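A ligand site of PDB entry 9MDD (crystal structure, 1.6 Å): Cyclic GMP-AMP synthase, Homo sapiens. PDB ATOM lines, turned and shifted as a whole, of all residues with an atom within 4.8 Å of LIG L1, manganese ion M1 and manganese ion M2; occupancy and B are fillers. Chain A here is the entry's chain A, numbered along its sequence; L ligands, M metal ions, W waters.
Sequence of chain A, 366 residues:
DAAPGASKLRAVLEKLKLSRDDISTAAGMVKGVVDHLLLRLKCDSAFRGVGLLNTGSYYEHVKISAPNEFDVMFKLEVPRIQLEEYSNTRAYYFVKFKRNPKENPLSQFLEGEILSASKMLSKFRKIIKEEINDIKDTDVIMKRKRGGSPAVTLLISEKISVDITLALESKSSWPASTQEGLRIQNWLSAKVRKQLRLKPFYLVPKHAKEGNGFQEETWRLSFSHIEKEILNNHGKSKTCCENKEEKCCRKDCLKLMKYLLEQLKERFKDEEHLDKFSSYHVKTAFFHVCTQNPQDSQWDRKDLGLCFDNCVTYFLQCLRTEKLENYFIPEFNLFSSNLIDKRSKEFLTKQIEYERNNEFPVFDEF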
ATOM      1  N   GLY A  56      25.716  19.565  -5.627  1.00  0.00           N
ATOM      2  CA  GLY A  56      25.689  18.266  -4.995  1.00  0.00           C
ATOM      3  C   GLY A  56      26.891  17.393  -5.336  1.00  0.00           C
ATOM      4  O   GLY A  56      27.843  17.799  -6.012  1.00  0.00           O
ATOM      5  N   SER A  57      26.819  16.146  -4.864  1.00  0.00           N
ATOM      6  CA  SER A  57      28.052  15.361  -4.726  1.00  0.00           C
ATOM      7  C   SER A  57      28.707  15.018  -6.060  1.00  0.00           C
ATOM      8  O   SER A  57      29.929  14.915  -6.133  1.00  0.00           O
ATOM      9  CB  SER A  57      27.775  14.082  -3.938  1.00  0.00           C
ATOM     10  OG  SER A  57      26.982  13.158  -4.677  1.00  0.00           O
ATOM     11  N   GLU A  60      30.772  17.934  -6.872  1.00  0.00           N
ATOM     12  CA  GLU A  60      31.785  18.072  -5.823  1.00  0.00           C
ATOM     13  C   GLU A  60      32.823  16.979  -5.898  1.00  0.00           C
ATOM     14  O   GLU A  60      33.789  17.014  -5.128  1.00  0.00           O
ATOM     15  CB  GLU A  60      31.135  18.028  -4.439  1.00  0.00           C
ATOM     16  CG  GLU A  60      30.206  19.208  -4.147  1.00  0.00           C
ATOM     17  CD  GLU A  60      29.282  18.959  -2.972  1.00  0.00           C
ATOM     18  OE1 GLU A  60      29.103  17.804  -2.525  1.00  0.00           O
ATOM     19  OE2 GLU A  60      28.718  19.966  -2.477  1.00  0.00           O
ATOM     20  N   VAL A  62      32.495  13.939  -4.914  1.00  0.00           N
ATOM     21  CA  VAL A  62      32.422  13.029  -3.764  1.00  0.00           C
ATOM     22  C   VAL A  62      31.198  12.112  -3.896  1.00  0.00           C
ATOM     23  O   VAL A  62      30.759  11.495  -2.912  1.00  0.00           O
ATOM     24  CB  VAL A  62      32.409  13.789  -2.419  1.00  0.00           C
ATOM     25  CG1 VAL A  62      33.748  14.507  -2.206  1.00  0.00           C
ATOM     26  CG2 VAL A  62      31.237  14.780  -2.331  1.00  0.00           C
ATOM     27  N   LYS A  63      30.678  11.965  -5.114  1.00  0.00           N
ATOM     28  CA  LYS A  63      29.712  10.910  -5.375  1.00  0.00           C
ATOM     29  C   LYS A  63      30.435   9.557  -5.342  1.00  0.00           C
ATOM     30  O   LYS A  63      31.483   9.399  -5.969  1.00  0.00           O
ATOM     31  CB  LYS A  63      29.055  11.125  -6.741  1.00  0.00           C
ATOM     32  CG  LYS A  63      28.044  10.020  -7.111  1.00  0.00           C
ATOM     33  CD  LYS A  63      26.678  10.294  -6.496  1.00  0.00           C
ATOM     34  CE  LYS A  63      25.704   9.142  -6.670  1.00  0.00           C
ATOM     35  NZ  LYS A  63      26.050   7.906  -5.907  1.00  0.00           N
ATOM     36  N   GLU A  69      23.002   9.523  -9.274  1.00  0.00           N
ATOM     37  CA  GLU A  69      22.169  10.527  -8.593  1.00  0.00           C
ATOM     38  C   GLU A  69      22.795  11.902  -8.796  1.00  0.00           C
ATOM     39  O   GLU A  69      23.935  12.170  -8.390  1.00  0.00           O
ATOM     40  CB  GLU A  69      22.032  10.210  -7.099  1.00  0.00           C
ATOM     41  CG  GLU A  69      20.733  10.817  -6.473  1.00  0.00           C
ATOM     42  CD  GLU A  69      20.923  12.196  -5.855  1.00  0.00           C
ATOM     43  OE1 GLU A  69      22.027  12.743  -5.956  1.00  0.00           O
ATOM     44  OE2 GLU A  69      19.932  12.709  -5.259  1.00  0.00           O
ATOM     45  N   ASP A  71      22.114  16.309  -8.911  1.00  0.00           N
ATOM     46  CA  ASP A  71      21.338  17.426  -8.391  1.00  0.00           C
ATOM     47  C   ASP A  71      21.561  18.662  -9.253  1.00  0.00           C
ATOM     48  O   ASP A  71      22.697  18.981  -9.575  1.00  0.00           O
ATOM     49  CB  ASP A  71      21.743  17.711  -6.945  1.00  0.00           C
ATOM     50  CG  ASP A  71      21.595  16.492  -6.080  1.00  0.00           C
ATOM     51  OD1 ASP A  71      20.442  16.093  -5.797  1.00  0.00           O
ATOM     52  OD2 ASP A  71      22.660  15.898  -5.730  1.00  0.00           O
ATOM     53  N   ARG A 146       8.512  13.072  -2.815  1.00  0.00           N
ATOM     54  CA  ARG A 146       9.337  12.648  -1.694  1.00  0.00           C
ATOM     55  C   ARG A 146       9.123  13.666  -0.585  1.00  0.00           C
ATOM     56  O   ARG A 146       9.498  14.837  -0.729  1.00  0.00           O
ATOM     57  CB  ARG A 146      10.806  12.570  -2.130  1.00  0.00           C
ATOM     58  CG  ARG A 146      11.823  12.076  -1.107  1.00  0.00           C
ATOM     59  CD  ARG A 146      13.180  11.800  -1.786  1.00  0.00           C
ATOM     60  NE  ARG A 146      13.770  13.009  -2.331  1.00  0.00           N
ATOM     61  CZ  ARG A 146      14.627  13.071  -3.350  1.00  0.00           C
ATOM     62  NH1 ARG A 146      14.989  11.987  -4.019  1.00  0.00           N
ATOM     63  NH2 ARG A 146      15.122  14.245  -3.715  1.00  0.00           N
ATOM     64  N   ASP A 163      17.550  15.122  -9.355  1.00  0.00           N
ATOM     65  CA  ASP A 163      16.729  16.011  -8.534  1.00  0.00           C
ATOM     66  C   ASP A 163      16.832  17.418  -9.094  1.00  0.00           C
ATOM     67  O   ASP A 163      17.908  18.019  -9.040  1.00  0.00           O
ATOM     68  CB  ASP A 163      17.184  16.024  -7.086  1.00  0.00           C
ATOM     69  CG  ASP A 163      16.936  14.726  -6.388  1.00  0.00           C
ATOM     70  OD1 ASP A 163      15.944  14.044  -6.681  1.00  0.00           O
ATOM     71  OD2 ASP A 163      17.713  14.415  -5.453  1.00  0.00           O
ATOM     72  N   ARG A 220      12.959  28.020   1.898  1.00  0.00           N
ATOM     73  CA  ARG A 220      14.103  27.730   2.752  1.00  0.00           C
ATOM     74  C   ARG A 220      15.397  28.153   2.082  1.00  0.00           C
ATOM     75  O   ARG A 220      15.562  28.001   0.866  1.00  0.00           O
ATOM     76  CB  ARG A 220      14.166  26.238   3.091  1.00  0.00           C
ATOM     77  CG  ARG A 220      15.323  25.899   4.038  1.00  0.00           C
ATOM     78  CD  ARG A 220      15.041  24.725   4.936  1.00  0.00           C
ATOM     79  NE  ARG A 220      16.289  24.108   5.372  1.00  0.00           N
ATOM     80  CZ  ARG A 220      16.384  23.052   6.173  1.00  0.00           C
ATOM     81  NH1 ARG A 220      15.308  22.505   6.725  1.00  0.00           N
ATOM     82  NH2 ARG A 220      17.576  22.511   6.406  1.00  0.00           N
ATOM     83  N   SER A 224      23.804  25.361  -1.280  1.00  0.00           N
ATOM     84  CA  SER A 224      24.402  24.225  -1.962  1.00  0.00           C
ATOM     85  C   SER A 224      25.521  24.684  -2.887  1.00  0.00           C
ATOM     86  O   SER A 224      26.545  23.988  -3.029  1.00  0.00           O
ATOM     87  CB  SER A 224      23.328  23.461  -2.750  1.00  0.00           C
ATOM     88  OG  SER A 224      23.804  22.218  -3.231  1.00  0.00           O
ATOM     89  N   GLU A 227      28.696  25.286  -0.823  1.00  0.00           N
ATOM     90  CA  GLU A 227      29.261  23.999  -0.443  1.00  0.00           C
ATOM     91  C   GLU A 227      30.118  23.434  -1.571  1.00  0.00           C
ATOM     92  O   GLU A 227      31.212  22.898  -1.329  1.00  0.00           O
ATOM     93  CB  GLU A 227      28.128  23.033  -0.099  1.00  0.00           C
ATOM     94  CG  GLU A 227      27.344  23.520   1.111  1.00  0.00           C
ATOM     95  CD  GLU A 227      26.021  22.801   1.309  1.00  0.00           C
ATOM     96  OE1 GLU A 227      25.776  21.771   0.625  1.00  0.00           O
ATOM     97  OE2 GLU A 227      25.197  23.316   2.108  1.00  0.00           O
ATOM     98  N   LYS A 258      30.235   9.242   4.183  1.00  0.00           N
ATOM     99  CA  LYS A 258      29.004   9.039   3.427  1.00  0.00           C
ATOM    100  C   LYS A 258      28.700   7.567   3.255  1.00  0.00           C
ATOM    101  O   LYS A 258      27.542   7.152   3.364  1.00  0.00           O
ATOM    102  CB  LYS A 258      29.108   9.722   2.057  1.00  0.00           C
ATOM    103  CG  LYS A 258      29.049  11.238   2.128  1.00  0.00           C
ATOM    104  CD  LYS A 258      29.293  11.874   0.772  1.00  0.00           C
ATOM    105  CE  LYS A 258      28.049  11.671  -0.118  1.00  0.00           C
ATOM    106  NZ  LYS A 258      28.275  12.215  -1.464  1.00  0.00           N
ATOM    107  N   SER A 278      20.596  11.819   6.744  1.00  0.00           N
ATOM    108  CA  SER A 278      20.935  11.883   5.338  1.00  0.00           C
ATOM    109  C   SER A 278      22.396  12.247   5.181  1.00  0.00           C
ATOM    110  O   SER A 278      23.094  12.591   6.151  1.00  0.00           O
ATOM    111  CB  SER A 278      20.084  12.908   4.570  1.00  0.00           C
ATOM    112  OG  SER A 278      20.554  14.217   4.798  1.00  0.00           O
ATOM    113  N   SER A 279      22.867  12.202   3.940  1.00  0.00           N
ATOM    114  CA  SER A 279      24.281  12.528   3.743  1.00  0.00           C
ATOM    115  C   SER A 279      24.579  13.981   4.096  1.00  0.00           C
ATOM    116  O   SER A 279      25.749  14.330   4.279  1.00  0.00           O
ATOM    117  CB  SER A 279      24.690  12.232   2.301  1.00  0.00           C
ATOM    118  OG  SER A 279      23.909  12.976   1.386  1.00  0.00           O
ATOM    119  N   TYR A 280      23.572  14.857   4.186  1.00  0.00           N
ATOM    120  CA  TYR A 280      23.859  16.232   4.588  1.00  0.00           C
ATOM    121  C   TYR A 280      24.282  16.316   6.043  1.00  0.00           C
ATOM    122  O   TYR A 280      25.023  17.236   6.420  1.00  0.00           O
ATOM    123  CB  TYR A 280      22.649  17.134   4.341  1.00  0.00           C
ATOM    124  CG  TYR A 280      23.022  18.601   4.354  1.00  0.00           C
ATOM    125  CD1 TYR A 280      23.808  19.150   3.341  1.00  0.00           C
ATOM    126  CD2 TYR A 280      22.601  19.433   5.401  1.00  0.00           C
ATOM    127  CE1 TYR A 280      24.179  20.478   3.364  1.00  0.00           C
ATOM    128  CE2 TYR A 280      22.963  20.771   5.406  1.00  0.00           C
ATOM    129  CZ  TYR A 280      23.751  21.289   4.385  1.00  0.00           C
ATOM    130  OH  TYR A 280      24.095  22.614   4.424  1.00  0.00           O
ATOM    131  N   LYS A 283      27.913  15.578   5.769  1.00  0.00           N
ATOM    132  CA  LYS A 283      28.550  16.698   5.087  1.00  0.00           C
ATOM    133  C   LYS A 283      28.738  17.885   6.029  1.00  0.00           C
ATOM    134  O   LYS A 283      29.814  18.513   6.051  1.00  0.00           O
ATOM    135  CB  LYS A 283      27.729  17.107   3.856  1.00  0.00           C
ATOM    136  CG  LYS A 283      28.460  18.013   2.876  1.00  0.00           C
ATOM    137  CD  LYS A 283      27.469  18.401   1.734  1.00  0.00           C
ATOM    138  CE  LYS A 283      28.161  19.092   0.586  1.00  0.00           C
ATOM    139  NZ  LYS A 283      27.153  19.591  -0.428  1.00  0.00           N
ATOM    140  N   ASN A 326      23.861  23.938  11.516  1.00  0.00           N
ATOM    141  CA  ASN A 326      24.012  24.173  10.091  1.00  0.00           C
ATOM    142  C   ASN A 326      25.246  25.060   9.866  1.00  0.00           C
ATOM    143  O   ASN A 326      25.495  26.003  10.609  1.00  0.00           O
ATOM    144  CB  ASN A 326      22.740  24.819   9.561  1.00  0.00           C
ATOM    145  CG  ASN A 326      22.802  25.104   8.072  1.00  0.00           C
ATOM    146  OD1 ASN A 326      23.452  26.054   7.638  1.00  0.00           O
ATOM    147  ND2 ASN A 326      22.114  24.275   7.278  1.00  0.00           N
HETATM  148  P1  LIG L   1      24.717  12.184  -2.266  1.00  0.00           P
HETATM  149  O1  LIG L   1      23.761  12.450  -3.401  1.00  0.00           O
HETATM  150  O2  LIG L   1      26.011  11.603  -2.848  1.00  0.00           O
HETATM  151  O3  LIG L   1      24.116  11.187  -1.200  1.00  0.00           O
HETATM  152  P2  LIG L   1      24.586  15.118  -1.935  1.00  0.00           P
HETATM  153  O4  LIG L   1      25.422  16.155  -1.261  1.00  0.00           O
HETATM  154  O5  LIG L   1      24.501  15.274  -3.469  1.00  0.00           O
HETATM  155  N1  LIG L   1      25.148  13.605  -1.463  1.00  0.00           N
HETATM  156  P3  LIG L   1      21.648  15.217  -1.806  1.00  0.00           P
HETATM  157  O6  LIG L   1      20.852  14.545  -0.743  1.00  0.00           O
HETATM  158  O7  LIG L   1      21.472  14.639  -3.235  1.00  0.00           O
HETATM  159  O8  LIG L   1      23.161  15.239  -1.282  1.00  0.00           O
HETATM  160  O9  LIG L   1      21.254  16.741  -1.769  1.00  0.00           O
HETATM  161  C1  LIG L   1      21.710  17.657  -2.770  1.00  0.00           C
HETATM  162  C2  LIG L   1      22.148  18.941  -2.084  1.00  0.00           C
HETATM  163  O10 LIG L   1      21.011  19.534  -1.429  1.00  0.00           O
HETATM  164  C3  LIG L   1      23.183  18.793  -0.967  1.00  0.00           C
HETATM  165  O11 LIG L   1      24.524  18.718  -1.447  1.00  0.00           O
HETATM  166  C4  LIG L   1      22.946  20.064  -0.157  1.00  0.00           C
HETATM  167  O12 LIG L   1      23.634  21.193  -0.695  1.00  0.00           O
HETATM  168  C5  LIG L   1      21.433  20.236  -0.265  1.00  0.00           C
HETATM  169  N2  LIG L   1      20.752  19.675   0.892  1.00  0.00           N
HETATM  170  C6  LIG L   1      20.360  18.378   1.093  1.00  0.00           C
HETATM  171  N3  LIG L   1      19.851  18.155   2.273  1.00  0.00           N
HETATM  172  C7  LIG L   1      19.900  19.389   2.900  1.00  0.00           C
HETATM  173  C8  LIG L   1      19.500  19.822   4.173  1.00  0.00           C
HETATM  174  N4  LIG L   1      18.950  19.029   5.101  1.00  0.00           N
HETATM  175  N5  LIG L   1      19.706  21.124   4.481  1.00  0.00           N
HETATM  176  C9  LIG L   1      20.282  21.922   3.578  1.00  0.00           C
HETATM  177  N6  LIG L   1      20.699  21.623   2.348  1.00  0.00           N
HETATM  178  C10 LIG L   1      20.477  20.332   2.071  1.00  0.00           C
HETATM  179  C1  LG2 L   2      15.949  17.892   1.698  1.00  0.00           C
HETATM  180  C2  LG2 L   2      17.737  20.106  -0.781  1.00  0.00           C
HETATM  181  C3  LG2 L   2      17.986  22.392  -0.052  1.00  0.00           C
HETATM  182  C4  LG2 L   2      16.963  20.709   1.391  1.00  0.00           C
HETATM  183  C5  LG2 L   2      19.492  21.673  -4.378  1.00  0.00           C
HETATM  184  C6  LG2 L   2      19.867  22.860  -3.792  1.00  0.00           C
HETATM  185  C7  LG2 L   2      17.751  15.275   1.408  1.00  0.00           C
HETATM  186  C8  LG2 L   2      17.975  16.022  -2.344  1.00  0.00           C
HETATM  187  C9  LG2 L   2      18.559  12.348  -2.392  1.00  0.00           C
HETATM  188  C10 LG2 L   2      17.834  14.530  -1.967  1.00  0.00           C
HETATM  189  C11 LG2 L   2      16.954  14.058  -0.932  1.00  0.00           C
HETATM  190  C12 LG2 L   2      16.949  12.693  -0.684  1.00  0.00           C
HETATM  191  C13 LG2 L   2      17.736  11.813  -1.393  1.00  0.00           C
HETATM  192  C14 LG2 L   2      16.066  14.966  -0.192  1.00  0.00           C
HETATM  193  C15 LG2 L   2      15.595  16.396   1.803  1.00  0.00           C
HETATM  194  C16 LG2 L   2      17.123  19.724   0.422  1.00  0.00           C
HETATM  195  C17 LG2 L   2      18.133  21.418  -1.015  1.00  0.00           C
HETATM  196  C18 LG2 L   2      17.400  21.988   1.114  1.00  0.00           C
HETATM  197  C19 LG2 L   2      18.762  21.796  -2.261  1.00  0.00           C
HETATM  198  C20 LG2 L   2      15.656  16.125   3.281  1.00  0.00           C
HETATM  199  N1  LG2 L   2      18.606  13.662  -2.646  1.00  0.00           N
HETATM  200  N2  LG2 L   2      16.462  15.538   1.019  1.00  0.00           N
HETATM  201  N3  LG2 L   2      16.730  18.372   0.619  1.00  0.00           N
HETATM  202  N4  LG2 L   2      18.762  20.999  -3.409  1.00  0.00           N
HETATM  203  N5  LG2 L   2      19.417  22.935  -2.482  1.00  0.00           N
HETATM  204  O1  LG2 L   2      15.576  18.624   2.580  1.00  0.00           O
HETATM  205  O2  LG2 L   2      14.977  15.168  -0.587  1.00  0.00           O
HETATM  206  O3  LG2 L   2      17.430  16.840  -1.589  1.00  0.00           O
HETATM  207  O4  LG2 L   2      18.634  16.229  -3.369  1.00  0.00           O
HETATM  208 CL1  LG2 L   2      17.196  23.214   2.352  1.00  0.00          CL
HETATM  209 MN    MN M   1      19.592  14.615  -4.454  1.00  0.00          MN
HETATM  210 MN    MN M   2      23.105  14.087  -4.645  1.00  0.00          MN
HETATM  211  O   HOH W   1      18.057  19.728   8.307  1.00  0.00           O
HETATM  212  O   HOH W   2      28.084  15.763  -1.025  1.00  0.00           O
HETATM  213  O   HOH W   3      21.591  11.741  -0.483  1.00  0.00           O
HETATM  214  O   HOH W   4      22.393  10.039  -3.776  1.00  0.00           O
HETATM  215  O   HOH W   5      21.641  15.005   1.850  1.00  0.00           O
HETATM  216  O   HOH W   6      24.818  13.699  -6.193  1.00  0.00           O
HETATM  217  O   HOH W   7      27.087   9.126  -3.258  1.00  0.00           O
HETATM  218  O   HOH W   8      20.317  21.977   7.271  1.00  0.00           O
HETATM  219  O   HOH W   9      24.528  16.040   1.504  1.00  0.00           O
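Manganese ion M2 is bound by the side-chain carboxylate (OD2) of Asp 71, an oxygen (O1) of LIG L1, the side-chain carboxylate (OE1) of Glu 69, an oxygen (O5) of LIG L1, an oxygen (O7) of LIG L1 and water W6. Manganese ion M2 has six donor atoms within binding distance.
Water W6 lies within hydrogen-bond range of OG of Ser 57 (2.7 Å) and O of Glu 69 (2.8 Å). Water W3 bridges an oxygen (O3) of LIG L1 (2.7 Å) and the side-chain hydroxyl (OG) of Ser 279 (3.2 Å). Water W2 lies within hydrogen-bond range of O4 of LIG L1 (2.7 Å) and OE1 of Glu 60 (2.7 Å). Water W9 lies within hydrogen-bond range of O4 of LIG L1 (2.9 Å), N of Tyr 280 (3.1 Å) and OG of Ser 279 (3.1 Å). Water W8 lies within hydrogen-bond range of ND2 of Asn 326, NH2 of Arg 220 and N5 of LIG L1. Water W1 bridges a nitrogen (N4) of LIG L1 (3.4 Å) and the guanidinium group of Arg 220 (3.4 Å).
NH2 of Arg 146 lies within salt-bridge range of OD1 of Asp 163 (3.1 Å). The side-chain carboxylate (OE1) of Glu 227 is in salt-bridge range of the side-chain amino group (NZ) of Lys 283 (2.8 Å). The side-chain carboxylate of Glu 227 is in hydrogen-bond range of the side-chain hydroxyl of Tyr 280. O of Ser 57 lies within hydrogen-bond range of N of Lys 63. N of Val 62 lies within hydrogen-bond range of O of Ser 57. The side-chain amino group (NZ) of Lys 258 sits at hydrogen-bond distance from the backbone carbonyl oxygen (O) of Val 62 (3.0 Å). The side-chain amino group of Lys 283 lies within salt-bridge range of the side-chain carboxylate of Glu 60. The side-chain hydroxyl (OG) of Ser 278 lies close to the backbone NH (N) of Tyr 280 (3.1 Å).
Manganese ion M1 is bound by OE2 of Glu 69 (2.1 Å), OD2 of Asp 163 (2.1 Å), O4 of LG2 L2 (2.2 Å), OD1 of Asp 71 (2.2 Å), O7 of LIG L1 (2.2 Å) and N1 of LG2 L2 (2.3 Å). Manganese ion M1 has six donor atoms within binding distance.
Ser 57 touches manganese ion M2. Of the 18 residues printed, 3 come within 4 Å of manganese ion M2. The nearest printed residue that does not touch manganese ion M2 is Gly 56 (4.9 Å).
Gly 56 touches LIG L1 (CA to O5, 3.6 Å). CD of Lys 63 touches O2 of LIG L1, 3.9 Å away. CD2 of Tyr 280 touches C8 of LIG L1, at 3.4 Å. The nearest printed residue that does not touch LIG L1 is Glu 60 (4.2 Å).
OE1 of Glu 227 sits at hydrogen-bond distance from O12 of LIG L1 (2.6 Å). An oxygen (O5) of LIG L1 lies close to the backbone NH (N) of Ser 57, 2.8 Å away. An oxygen (O2) of LIG L1 lies within hydrogen-bond range of the side-chain hydroxyl (OG) of Ser 57. The side-chain amino group (NZ) of Lys 258 is in salt-bridge range of an oxygen (O2) of LIG L1, at 2.7 Å. The side-chain hydroxyl (OG) of Ser 224 is in hydrogen-bond range of an oxygen (O12) of LIG L1. The side-chain amino group of Lys 283 is in salt-bridge range of an oxygen (O4) of LIG L1 (3.9 Å). The side-chain hydroxyl of Ser 279 lies within hydrogen-bond range of an oxygen (O3) of LIG L1, at 3.2 Å. The guanidinium group (NH2) of Arg 220 lies within hydrogen-bond range of a nitrogen (N5) of LIG L1 (3.2 Å). An oxygen (O2) of LG2 L2 sits at hydrogen-bond distance from the guanidinium group (NE) of Arg 146, 3.0 Å away.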
